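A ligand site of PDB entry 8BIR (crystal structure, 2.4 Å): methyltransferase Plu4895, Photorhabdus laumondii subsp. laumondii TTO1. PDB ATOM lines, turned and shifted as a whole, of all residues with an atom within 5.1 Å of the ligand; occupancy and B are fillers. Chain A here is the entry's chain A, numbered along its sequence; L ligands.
S1 of the ligand sits close to ND2 of Asn 248, 3.8 Å away.
N of Phe 229 sits at hydrogen-bond distance from N5 of the ligand (3.0 Å).
OD2 of Asp 228 lies within hydrogen-bond range of N4 of the ligand (2.6 Å).
An oxygen (O2) of the ligand is in salt-bridge range of the side-chain amino group of Lys 243.
N1 of the ligand lies within hydrogen-bond range of O of Gly 188.
O of Lys 243 sits at hydrogen-bond distance from N1 of the ligand, 2.5 Å away.
An oxygen (O5) of the ligand sits at hydrogen-bond distance from the side-chain carboxylate (OD1) of Asp 211 (2.5 Å).
The side-chain amide nitrogen of Asn 248 lies within hydrogen-bond range of the backbone carbonyl oxygen of Asn 244, at 3.3 Å.
The side-chain carboxylate of Asp 211 is in hydrogen-bond range of the backbone NH of Gly 190 (2.8 Å).
The backbone carbonyl oxygen (O) of Leu 210 sits at hydrogen-bond distance from the backbone NH (N) of Gly 188, 2.8 Å away.
The side-chain carboxylate of Asp 228 is in hydrogen-bond range of the backbone NH of Phe 230.
NZ of Lys 243 lies close to ND2 of Asn 244, 3.4 Å away.
The backbone NH (N) of Gly 189 is in hydrogen-bond range of the side-chain carboxylate (OD2) of Asp 211 (3.2 Å).
O of Asn 244 sits close to S1 of the ligand, at 3.4 Å.
CE1 of Phe 144 touches C8 of the ligand, 3.6 Å away.
CZ of Phe 157 touches S1 of the ligand (3.6 Å).
CB of Met 161 touches O1 of the ligand, at 3.9 Å.
Thr 165 touches the ligand (CG2 to O1, 3.3 Å).
Gly 189 touches the ligand (CA to N1, 3.8 Å).
N of Gly 190 touches O4 of the ligand, at 3.95 Å.
Phe 230 touches the ligand.
CZ2 of Trp 249 touches N3 of the ligand, 3.8 Å away.
Hydrophobic or aromatic side chains that line the ligand: Phe 144, Phe 157, Met 161, Phe 229, Phe 230 and Trp 249.
15 residues have an atom within 4 Å of the ligand: Phe 144, Phe 157, Met 161, Thr 165, Gly 188, Gly 189, Gly 190, Asp 211, Asp 228, Phe 229, Phe 230, Lys 243, Asn 244, Asn 248 and Trp 249.
Along chain A the residues within 4 Å of the ligand span positions 144 to 249.
The nearest printed residue that does not touch the ligand is Val 245 (4.1 Å).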
ATOM      1  N   PHE A 144      21.920  13.521   5.487  1.00  0.00           N
ATOM      2  CA  PHE A 144      20.457  13.783   5.525  1.00  0.00           C
ATOM      3  C   PHE A 144      19.872  13.327   6.873  1.00  0.00           C
ATOM      4  O   PHE A 144      18.919  13.976   7.341  1.00  0.00           O
ATOM      5  CB  PHE A 144      19.762  13.132   4.329  1.00  0.00           C
ATOM      6  CG  PHE A 144      19.989  13.850   3.033  1.00  0.00           C
ATOM      7  CD1 PHE A 144      19.636  15.180   2.893  1.00  0.00           C
ATOM      8  CD2 PHE A 144      20.553  13.204   1.937  1.00  0.00           C
ATOM      9  CE1 PHE A 144      19.840  15.856   1.697  1.00  0.00           C
ATOM     10  CE2 PHE A 144      20.757  13.880   0.741  1.00  0.00           C
ATOM     11  CZ  PHE A 144      20.406  15.200   0.621  1.00  0.00           C
ATOM     12  N   LYS A 154      18.633  22.386   7.995  1.00  0.00           N
ATOM     13  CA  LYS A 154      17.684  21.887   6.962  1.00  0.00           C
ATOM     14  C   LYS A 154      16.968  23.078   6.299  1.00  0.00           C
ATOM     15  O   LYS A 154      16.873  23.085   5.060  1.00  0.00           O
ATOM     16  CB  LYS A 154      16.666  20.926   7.570  1.00  0.00           C
ATOM     17  CG  LYS A 154      15.585  20.441   6.607  1.00  0.00           C
ATOM     18  CD  LYS A 154      14.940  19.125   6.998  1.00  0.00           C
ATOM     19  CE  LYS A 154      13.988  18.605   5.940  1.00  0.00           C
ATOM     20  NZ  LYS A 154      13.491  17.241   6.262  1.00  0.00           N
ATOM     21  N   PHE A 157      19.548  24.781   4.268  1.00  0.00           N
ATOM     22  CA  PHE A 157      19.773  23.904   3.089  1.00  0.00           C
ATOM     23  C   PHE A 157      18.686  24.173   2.041  1.00  0.00           C
ATOM     24  O   PHE A 157      19.029  24.534   0.898  1.00  0.00           O
ATOM     25  CB  PHE A 157      19.793  22.432   3.515  1.00  0.00           C
ATOM     26  CG  PHE A 157      19.861  21.429   2.391  1.00  0.00           C
ATOM     27  CD1 PHE A 157      21.061  21.137   1.777  1.00  0.00           C
ATOM     28  CD2 PHE A 157      18.712  20.783   1.947  1.00  0.00           C
ATOM     29  CE1 PHE A 157      21.119  20.212   0.740  1.00  0.00           C
ATOM     30  CE2 PHE A 157      18.779  19.857   0.914  1.00  0.00           C
ATOM     31  CZ  PHE A 157      19.979  19.583   0.309  1.00  0.00           C
ATOM     32  N   ASP A 158      17.416  24.023   2.434  1.00  0.00           N
ATOM     33  CA  ASP A 158      16.227  24.233   1.577  1.00  0.00           C
ATOM     34  C   ASP A 158      16.243  25.667   1.011  1.00  0.00           C
ATOM     35  O   ASP A 158      15.984  25.808  -0.195  1.00  0.00           O
ATOM     36  CB  ASP A 158      14.928  23.957   2.341  1.00  0.00           C
ATOM     37  CG  ASP A 158      14.596  22.477   2.468  1.00  0.00           C
ATOM     38  OD1 ASP A 158      14.562  21.800   1.425  1.00  0.00           O
ATOM     39  OD2 ASP A 158      14.358  22.030   3.612  1.00  0.00           O
ATOM     40  N   MET A 161      18.880  25.877  -1.678  1.00  0.00           N
ATOM     41  CA  MET A 161      18.394  25.022  -2.790  1.00  0.00           C
ATOM     42  C   MET A 161      17.295  25.776  -3.557  1.00  0.00           C
ATOM     43  O   MET A 161      17.334  25.744  -4.794  1.00  0.00           O
ATOM     44  CB  MET A 161      17.846  23.680  -2.295  1.00  0.00           C
ATOM     45  CG  MET A 161      18.927  22.733  -1.787  1.00  0.00           C
ATOM     46  SD  MET A 161      20.145  22.285  -3.054  1.00  0.00           S
ATOM     47  CE  MET A 161      21.651  22.304  -2.088  1.00  0.00           C
ATOM     48  N   THR A 165      16.716  26.537  -7.917  1.00  0.00           N
ATOM     49  CA  THR A 165      15.490  26.165  -8.677  1.00  0.00           C
ATOM     50  C   THR A 165      14.946  27.416  -9.376  1.00  0.00           C
ATOM     51  O   THR A 165      14.602  27.319 -10.565  1.00  0.00           O
ATOM     52  CB  THR A 165      14.429  25.494  -7.784  1.00  0.00           C
ATOM     53  OG1 THR A 165      13.741  26.521  -7.065  1.00  0.00           O
ATOM     54  CG2 THR A 165      14.992  24.485  -6.811  1.00  0.00           C
ATOM     55  N   ASP A 186       7.344  15.187  -7.827  1.00  0.00           N
ATOM     56  CA  ASP A 186       8.745  15.648  -7.613  1.00  0.00           C
ATOM     57  C   ASP A 186       9.366  14.848  -6.452  1.00  0.00           C
ATOM     58  O   ASP A 186       9.001  15.108  -5.291  1.00  0.00           O
ATOM     59  CB  ASP A 186       8.800  17.155  -7.362  1.00  0.00           C
ATOM     60  CG  ASP A 186      10.203  17.730  -7.281  1.00  0.00           C
ATOM     61  OD1 ASP A 186      11.116  17.148  -7.902  1.00  0.00           O
ATOM     62  OD2 ASP A 186      10.374  18.764  -6.607  1.00  0.00           O
ATOM     63  N   LEU A 187      10.279  13.922  -6.781  1.00  0.00           N
ATOM     64  CA  LEU A 187      10.929  13.005  -5.805  1.00  0.00           C
ATOM     65  C   LEU A 187      12.168  13.699  -5.208  1.00  0.00           C
ATOM     66  O   LEU A 187      13.010  14.181  -5.996  1.00  0.00           O
ATOM     67  CB  LEU A 187      11.310  11.707  -6.529  1.00  0.00           C
ATOM     68  CG  LEU A 187      10.130  10.892  -7.041  1.00  0.00           C
ATOM     69  CD1 LEU A 187      10.579   9.889  -8.089  1.00  0.00           C
ATOM     70  CD2 LEU A 187       9.422  10.186  -5.896  1.00  0.00           C
ATOM     71  N   GLY A 188      12.249  13.756  -3.878  1.00  0.00           N
ATOM     72  CA  GLY A 188      13.260  14.532  -3.133  1.00  0.00           C
ATOM     73  C   GLY A 188      13.185  16.004  -3.498  1.00  0.00           C
ATOM     74  O   GLY A 188      14.226  16.556  -3.926  1.00  0.00           O
ATOM     75  N   GLY A 189      12.003  16.609  -3.355  1.00  0.00           N
ATOM     76  CA  GLY A 189      11.711  17.999  -3.778  1.00  0.00           C
ATOM     77  C   GLY A 189      11.839  18.989  -2.634  1.00  0.00           C
ATOM     78  O   GLY A 189      11.828  20.201  -2.927  1.00  0.00           O
ATOM     79  N   GLY A 190      11.959  18.509  -1.393  1.00  0.00           N
ATOM     80  CA  GLY A 190      11.959  19.340  -0.172  1.00  0.00           C
ATOM     81  C   GLY A 190      10.725  20.218  -0.126  1.00  0.00           C
ATOM     82  O   GLY A 190       9.611  19.681  -0.275  1.00  0.00           O
ATOM     83  N   LEU A 210       7.270  14.449  -2.896  1.00  0.00           N
ATOM     84  CA  LEU A 210       7.658  13.340  -1.984  1.00  0.00           C
ATOM     85  C   LEU A 210       9.058  13.635  -1.431  1.00  0.00           C
ATOM     86  O   LEU A 210       9.971  13.874  -2.245  1.00  0.00           O
ATOM     87  CB  LEU A 210       7.620  12.013  -2.755  1.00  0.00           C
ATOM     88  CG  LEU A 210       7.417  10.762  -1.907  1.00  0.00           C
ATOM     89  CD1 LEU A 210       6.972   9.588  -2.769  1.00  0.00           C
ATOM     90  CD2 LEU A 210       8.680  10.397  -1.136  1.00  0.00           C
ATOM     91  N   ASP A 211       9.203  13.617  -0.101  1.00  0.00           N
ATOM     92  CA  ASP A 211      10.484  13.871   0.609  1.00  0.00           C
ATOM     93  C   ASP A 211      10.323  13.497   2.096  1.00  0.00           C
ATOM     94  O   ASP A 211       9.165  13.406   2.560  1.00  0.00           O
ATOM     95  CB  ASP A 211      10.920  15.333   0.459  1.00  0.00           C
ATOM     96  CG  ASP A 211      12.421  15.545   0.596  1.00  0.00           C
ATOM     97  OD1 ASP A 211      12.991  15.067   1.589  1.00  0.00           O
ATOM     98  OD2 ASP A 211      13.003  16.193  -0.295  1.00  0.00           O
ATOM     99  N   ARG A 212      11.431  13.295   2.799  1.00  0.00           N
ATOM    100  CA  ARG A 212      11.467  13.041   4.270  1.00  0.00           C
ATOM    101  C   ARG A 212      11.234  14.359   5.011  1.00  0.00           C
ATOM    102  O   ARG A 212      12.185  15.170   5.098  1.00  0.00           O
ATOM    103  CB  ARG A 212      12.810  12.429   4.699  1.00  0.00           C
ATOM    104  CG  ARG A 212      12.885  10.911   4.586  1.00  0.00           C
ATOM    105  CD  ARG A 212      13.789  10.340   5.658  1.00  0.00           C
ATOM    106  NE  ARG A 212      14.049   8.913   5.519  1.00  0.00           N
ATOM    107  CZ  ARG A 212      14.774   8.186   6.375  1.00  0.00           C
ATOM    108  NH1 ARG A 212      15.324   8.746   7.430  1.00  0.00           N
ATOM    109  NH2 ARG A 212      14.947   6.891   6.146  1.00  0.00           N
ATOM    110  N   GLY A 227       7.342  10.215   2.528  1.00  0.00           N
ATOM    111  CA  GLY A 227       7.802   8.835   2.249  1.00  0.00           C
ATOM    112  C   GLY A 227       9.293   8.761   1.982  1.00  0.00           C
ATOM    113  O   GLY A 227      10.007   9.747   2.253  1.00  0.00           O
ATOM    114  N   ASP A 228       9.746   7.606   1.467  1.00  0.00           N
ATOM    115  CA  ASP A 228      11.163   7.281   1.154  1.00  0.00           C
ATOM    116  C   ASP A 228      11.229   6.698  -0.258  1.00  0.00           C
ATOM    117  O   ASP A 228      10.477   5.735  -0.534  1.00  0.00           O
ATOM    118  CB  ASP A 228      11.723   6.318   2.211  1.00  0.00           C
ATOM    119  CG  ASP A 228      13.097   5.736   1.911  1.00  0.00           C
ATOM    120  OD1 ASP A 228      13.484   4.768   2.593  1.00  0.00           O
ATOM    121  OD2 ASP A 228      13.768   6.256   0.991  1.00  0.00           O
ATOM    122  N   PHE A 229      12.089   7.244  -1.126  1.00  0.00           N
ATOM    123  CA  PHE A 229      12.181   6.894  -2.572  1.00  0.00           C
ATOM    124  C   PHE A 229      13.056   5.647  -2.785  1.00  0.00           C
ATOM    125  O   PHE A 229      13.337   5.318  -3.950  1.00  0.00           O
ATOM    126  CB  PHE A 229      12.644   8.079  -3.422  1.00  0.00           C
ATOM    127  CG  PHE A 229      13.936   8.758  -3.030  1.00  0.00           C
ATOM    128  CD1 PHE A 229      15.005   8.059  -2.479  1.00  0.00           C
ATOM    129  CD2 PHE A 229      14.105  10.124  -3.256  1.00  0.00           C
ATOM    130  CE1 PHE A 229      16.180   8.701  -2.136  1.00  0.00           C
ATOM    131  CE2 PHE A 229      15.280  10.757  -2.917  1.00  0.00           C
ATOM    132  CZ  PHE A 229      16.314  10.053  -2.360  1.00  0.00           C
ATOM    133  N   PHE A 230      13.487   4.988  -1.696  1.00  0.00           N
ATOM    134  CA  PHE A 230      14.138   3.653  -1.717  1.00  0.00           C
ATOM    135  C   PHE A 230      13.063   2.555  -1.673  1.00  0.00           C
ATOM    136  O   PHE A 230      13.403   1.378  -1.897  1.00  0.00           O
ATOM    137  CB  PHE A 230      15.140   3.508  -0.566  1.00  0.00           C
ATOM    138  CG  PHE A 230      16.417   4.282  -0.729  1.00  0.00           C
ATOM    139  CD1 PHE A 230      17.218   4.108  -1.842  1.00  0.00           C
ATOM    140  CD2 PHE A 230      16.824   5.186   0.239  1.00  0.00           C
ATOM    141  CE1 PHE A 230      18.396   4.827  -1.994  1.00  0.00           C
ATOM    142  CE2 PHE A 230      18.002   5.905   0.087  1.00  0.00           C
ATOM    143  CZ  PHE A 230      18.791   5.727  -1.021  1.00  0.00           C
ATOM    144  N   LYS A 243      15.485  16.181  -9.237  1.00  0.00           N
ATOM    145  CA  LYS A 243      16.320  17.406  -9.394  1.00  0.00           C
ATOM    146  C   LYS A 243      17.360  17.465  -8.264  1.00  0.00           C
ATOM    147  O   LYS A 243      16.936  17.601  -7.110  1.00  0.00           O
ATOM    148  CB  LYS A 243      15.435  18.661  -9.413  1.00  0.00           C
ATOM    149  CG  LYS A 243      16.172  19.947  -9.717  1.00  0.00           C
ATOM    150  CD  LYS A 243      15.335  21.196  -9.547  1.00  0.00           C
ATOM    151  CE  LYS A 243      16.175  22.459  -9.559  1.00  0.00           C
ATOM    152  NZ  LYS A 243      17.212  22.445  -8.506  1.00  0.00           N
ATOM    153  N   ASN A 244      18.654  17.379  -8.614  1.00  0.00           N
ATOM    154  CA  ASN A 244      19.799  17.409  -7.659  1.00  0.00           C
ATOM    155  C   ASN A 244      19.587  16.338  -6.571  1.00  0.00           C
ATOM    156  O   ASN A 244      19.707  16.682  -5.376  1.00  0.00           O
ATOM    157  CB  ASN A 244      20.000  18.790  -7.042  1.00  0.00           C
ATOM    158  CG  ASN A 244      20.662  19.781  -7.980  1.00  0.00           C
ATOM    159  OD1 ASN A 244      21.568  19.422  -8.729  1.00  0.00           O
ATOM    160  ND2 ASN A 244      20.235  21.031  -7.928  1.00  0.00           N
ATOM    161  N   VAL A 245      19.275  15.111  -6.972  1.00  0.00           N
ATOM    162  CA  VAL A 245      19.009  13.961  -6.062  1.00  0.00           C
ATOM    163  C   VAL A 245      20.028  12.847  -6.346  1.00  0.00           C
ATOM    164  O   VAL A 245      20.621  12.344  -5.368  1.00  0.00           O
ATOM    165  CB  VAL A 245      17.558  13.453  -6.190  1.00  0.00           C
ATOM    166  CG1 VAL A 245      17.328  12.163  -5.399  1.00  0.00           C
ATOM    167  CG2 VAL A 245      16.564  14.516  -5.762  1.00  0.00           C
ATOM    168  N   ASN A 248      23.603  12.974  -5.015  1.00  0.00           N
ATOM    169  CA  ASN A 248      23.717  12.754  -3.539  1.00  0.00           C
ATOM    170  C   ASN A 248      23.995  11.285  -3.226  1.00  0.00           C
ATOM    171  O   ASN A 248      24.089  10.958  -2.025  1.00  0.00           O
ATOM    172  CB  ASN A 248      22.442  13.166  -2.795  1.00  0.00           C
ATOM    173  CG  ASN A 248      22.088  14.624  -2.940  1.00  0.00           C
ATOM    174  OD1 ASN A 248      22.957  15.460  -3.170  1.00  0.00           O
ATOM    175  ND2 ASN A 248      20.819  14.950  -2.791  1.00  0.00           N
ATOM    176  N   TRP A 249      24.085  10.418  -4.241  1.00  0.00           N
ATOM    177  CA  TRP A 249      24.137   8.936  -4.076  1.00  0.00           C
ATOM    178  C   TRP A 249      25.177   8.333  -5.017  1.00  0.00           C
ATOM    179  O   TRP A 249      25.376   8.838  -6.123  1.00  0.00           O
ATOM    180  CB  TRP A 249      22.750   8.325  -4.303  1.00  0.00           C
ATOM    181  CG  TRP A 249      21.688   8.891  -3.404  1.00  0.00           C
ATOM    182  CD1 TRP A 249      20.753   9.820  -3.732  1.00  0.00           C
ATOM    183  CD2 TRP A 249      21.477   8.578  -2.016  1.00  0.00           C
ATOM    184  NE1 TRP A 249      19.960  10.095  -2.660  1.00  0.00           N
ATOM    185  CE2 TRP A 249      20.374   9.344  -1.590  1.00  0.00           C
ATOM    186  CE3 TRP A 249      22.093   7.713  -1.100  1.00  0.00           C
ATOM    187  CZ2 TRP A 249      19.887   9.296  -0.283  1.00  0.00           C
ATOM    188  CZ3 TRP A 249      21.610   7.653   0.190  1.00  0.00           C
ATOM    189  CH2 TRP A 249      20.519   8.432   0.591  1.00  0.00           C
HETATM  190  N1  LIG L   1      15.074  18.346  -5.560  1.00  0.00           N
HETATM  191  C1  LIG L   1      15.293  19.516  -4.644  1.00  0.00           C
HETATM  192  C2  LIG L   1      16.239  19.161  -3.486  1.00  0.00           C
HETATM  193  C3  LIG L   1      17.402  18.248  -3.841  1.00  0.00           C
HETATM  194  S1  LIG L   1      18.402  17.796  -2.405  1.00  0.00           S
HETATM  195  C4  LIG L   1      15.868  20.684  -5.453  1.00  0.00           C
HETATM  196  O1  LIG L   1      15.833  21.842  -5.015  1.00  0.00           O
HETATM  197  O2  LIG L   1      16.377  20.525  -6.556  1.00  0.00           O
HETATM  198  C5  LIG L   1      17.997  16.057  -2.132  1.00  0.00           C
HETATM  199  C6  LIG L   1      16.690  15.789  -1.428  1.00  0.00           C
HETATM  200  O3  LIG L   1      16.518  14.367  -1.246  1.00  0.00           O
HETATM  201  C7  LIG L   1      16.562  16.413  -0.035  1.00  0.00           C
HETATM  202  O4  LIG L   1      15.444  17.294   0.017  1.00  0.00           O
HETATM  203  C8  LIG L   1      16.355  15.217   0.902  1.00  0.00           C
HETATM  204  O5  LIG L   1      15.450  15.476   1.952  1.00  0.00           O
HETATM  205  C9  LIG L   1      15.793  14.167  -0.056  1.00  0.00           C
HETATM  206  N2  LIG L   1      15.951  12.785   0.383  1.00  0.00           N
HETATM  207  C10 LIG L   1      17.028  12.229   1.027  1.00  0.00           C
HETATM  208  N3  LIG L   1      16.867  10.955   1.294  1.00  0.00           N
HETATM  209  C11 LIG L   1      15.602  10.652   0.810  1.00  0.00           C
HETATM  210  C12 LIG L   1      14.854   9.459   0.805  1.00  0.00           C
HETATM  211  N4  LIG L   1      15.294   8.307   1.302  1.00  0.00           N
HETATM  212  N5  LIG L   1      13.630   9.498   0.231  1.00  0.00           N
HETATM  213  C13 LIG L   1      13.194  10.662  -0.270  1.00  0.00           C
HETATM  214  N6  LIG L   1      13.809  11.844  -0.318  1.00  0.00           N
HETATM  215  C14 LIG L   1      15.021  11.775   0.246  1.00  0.00           C
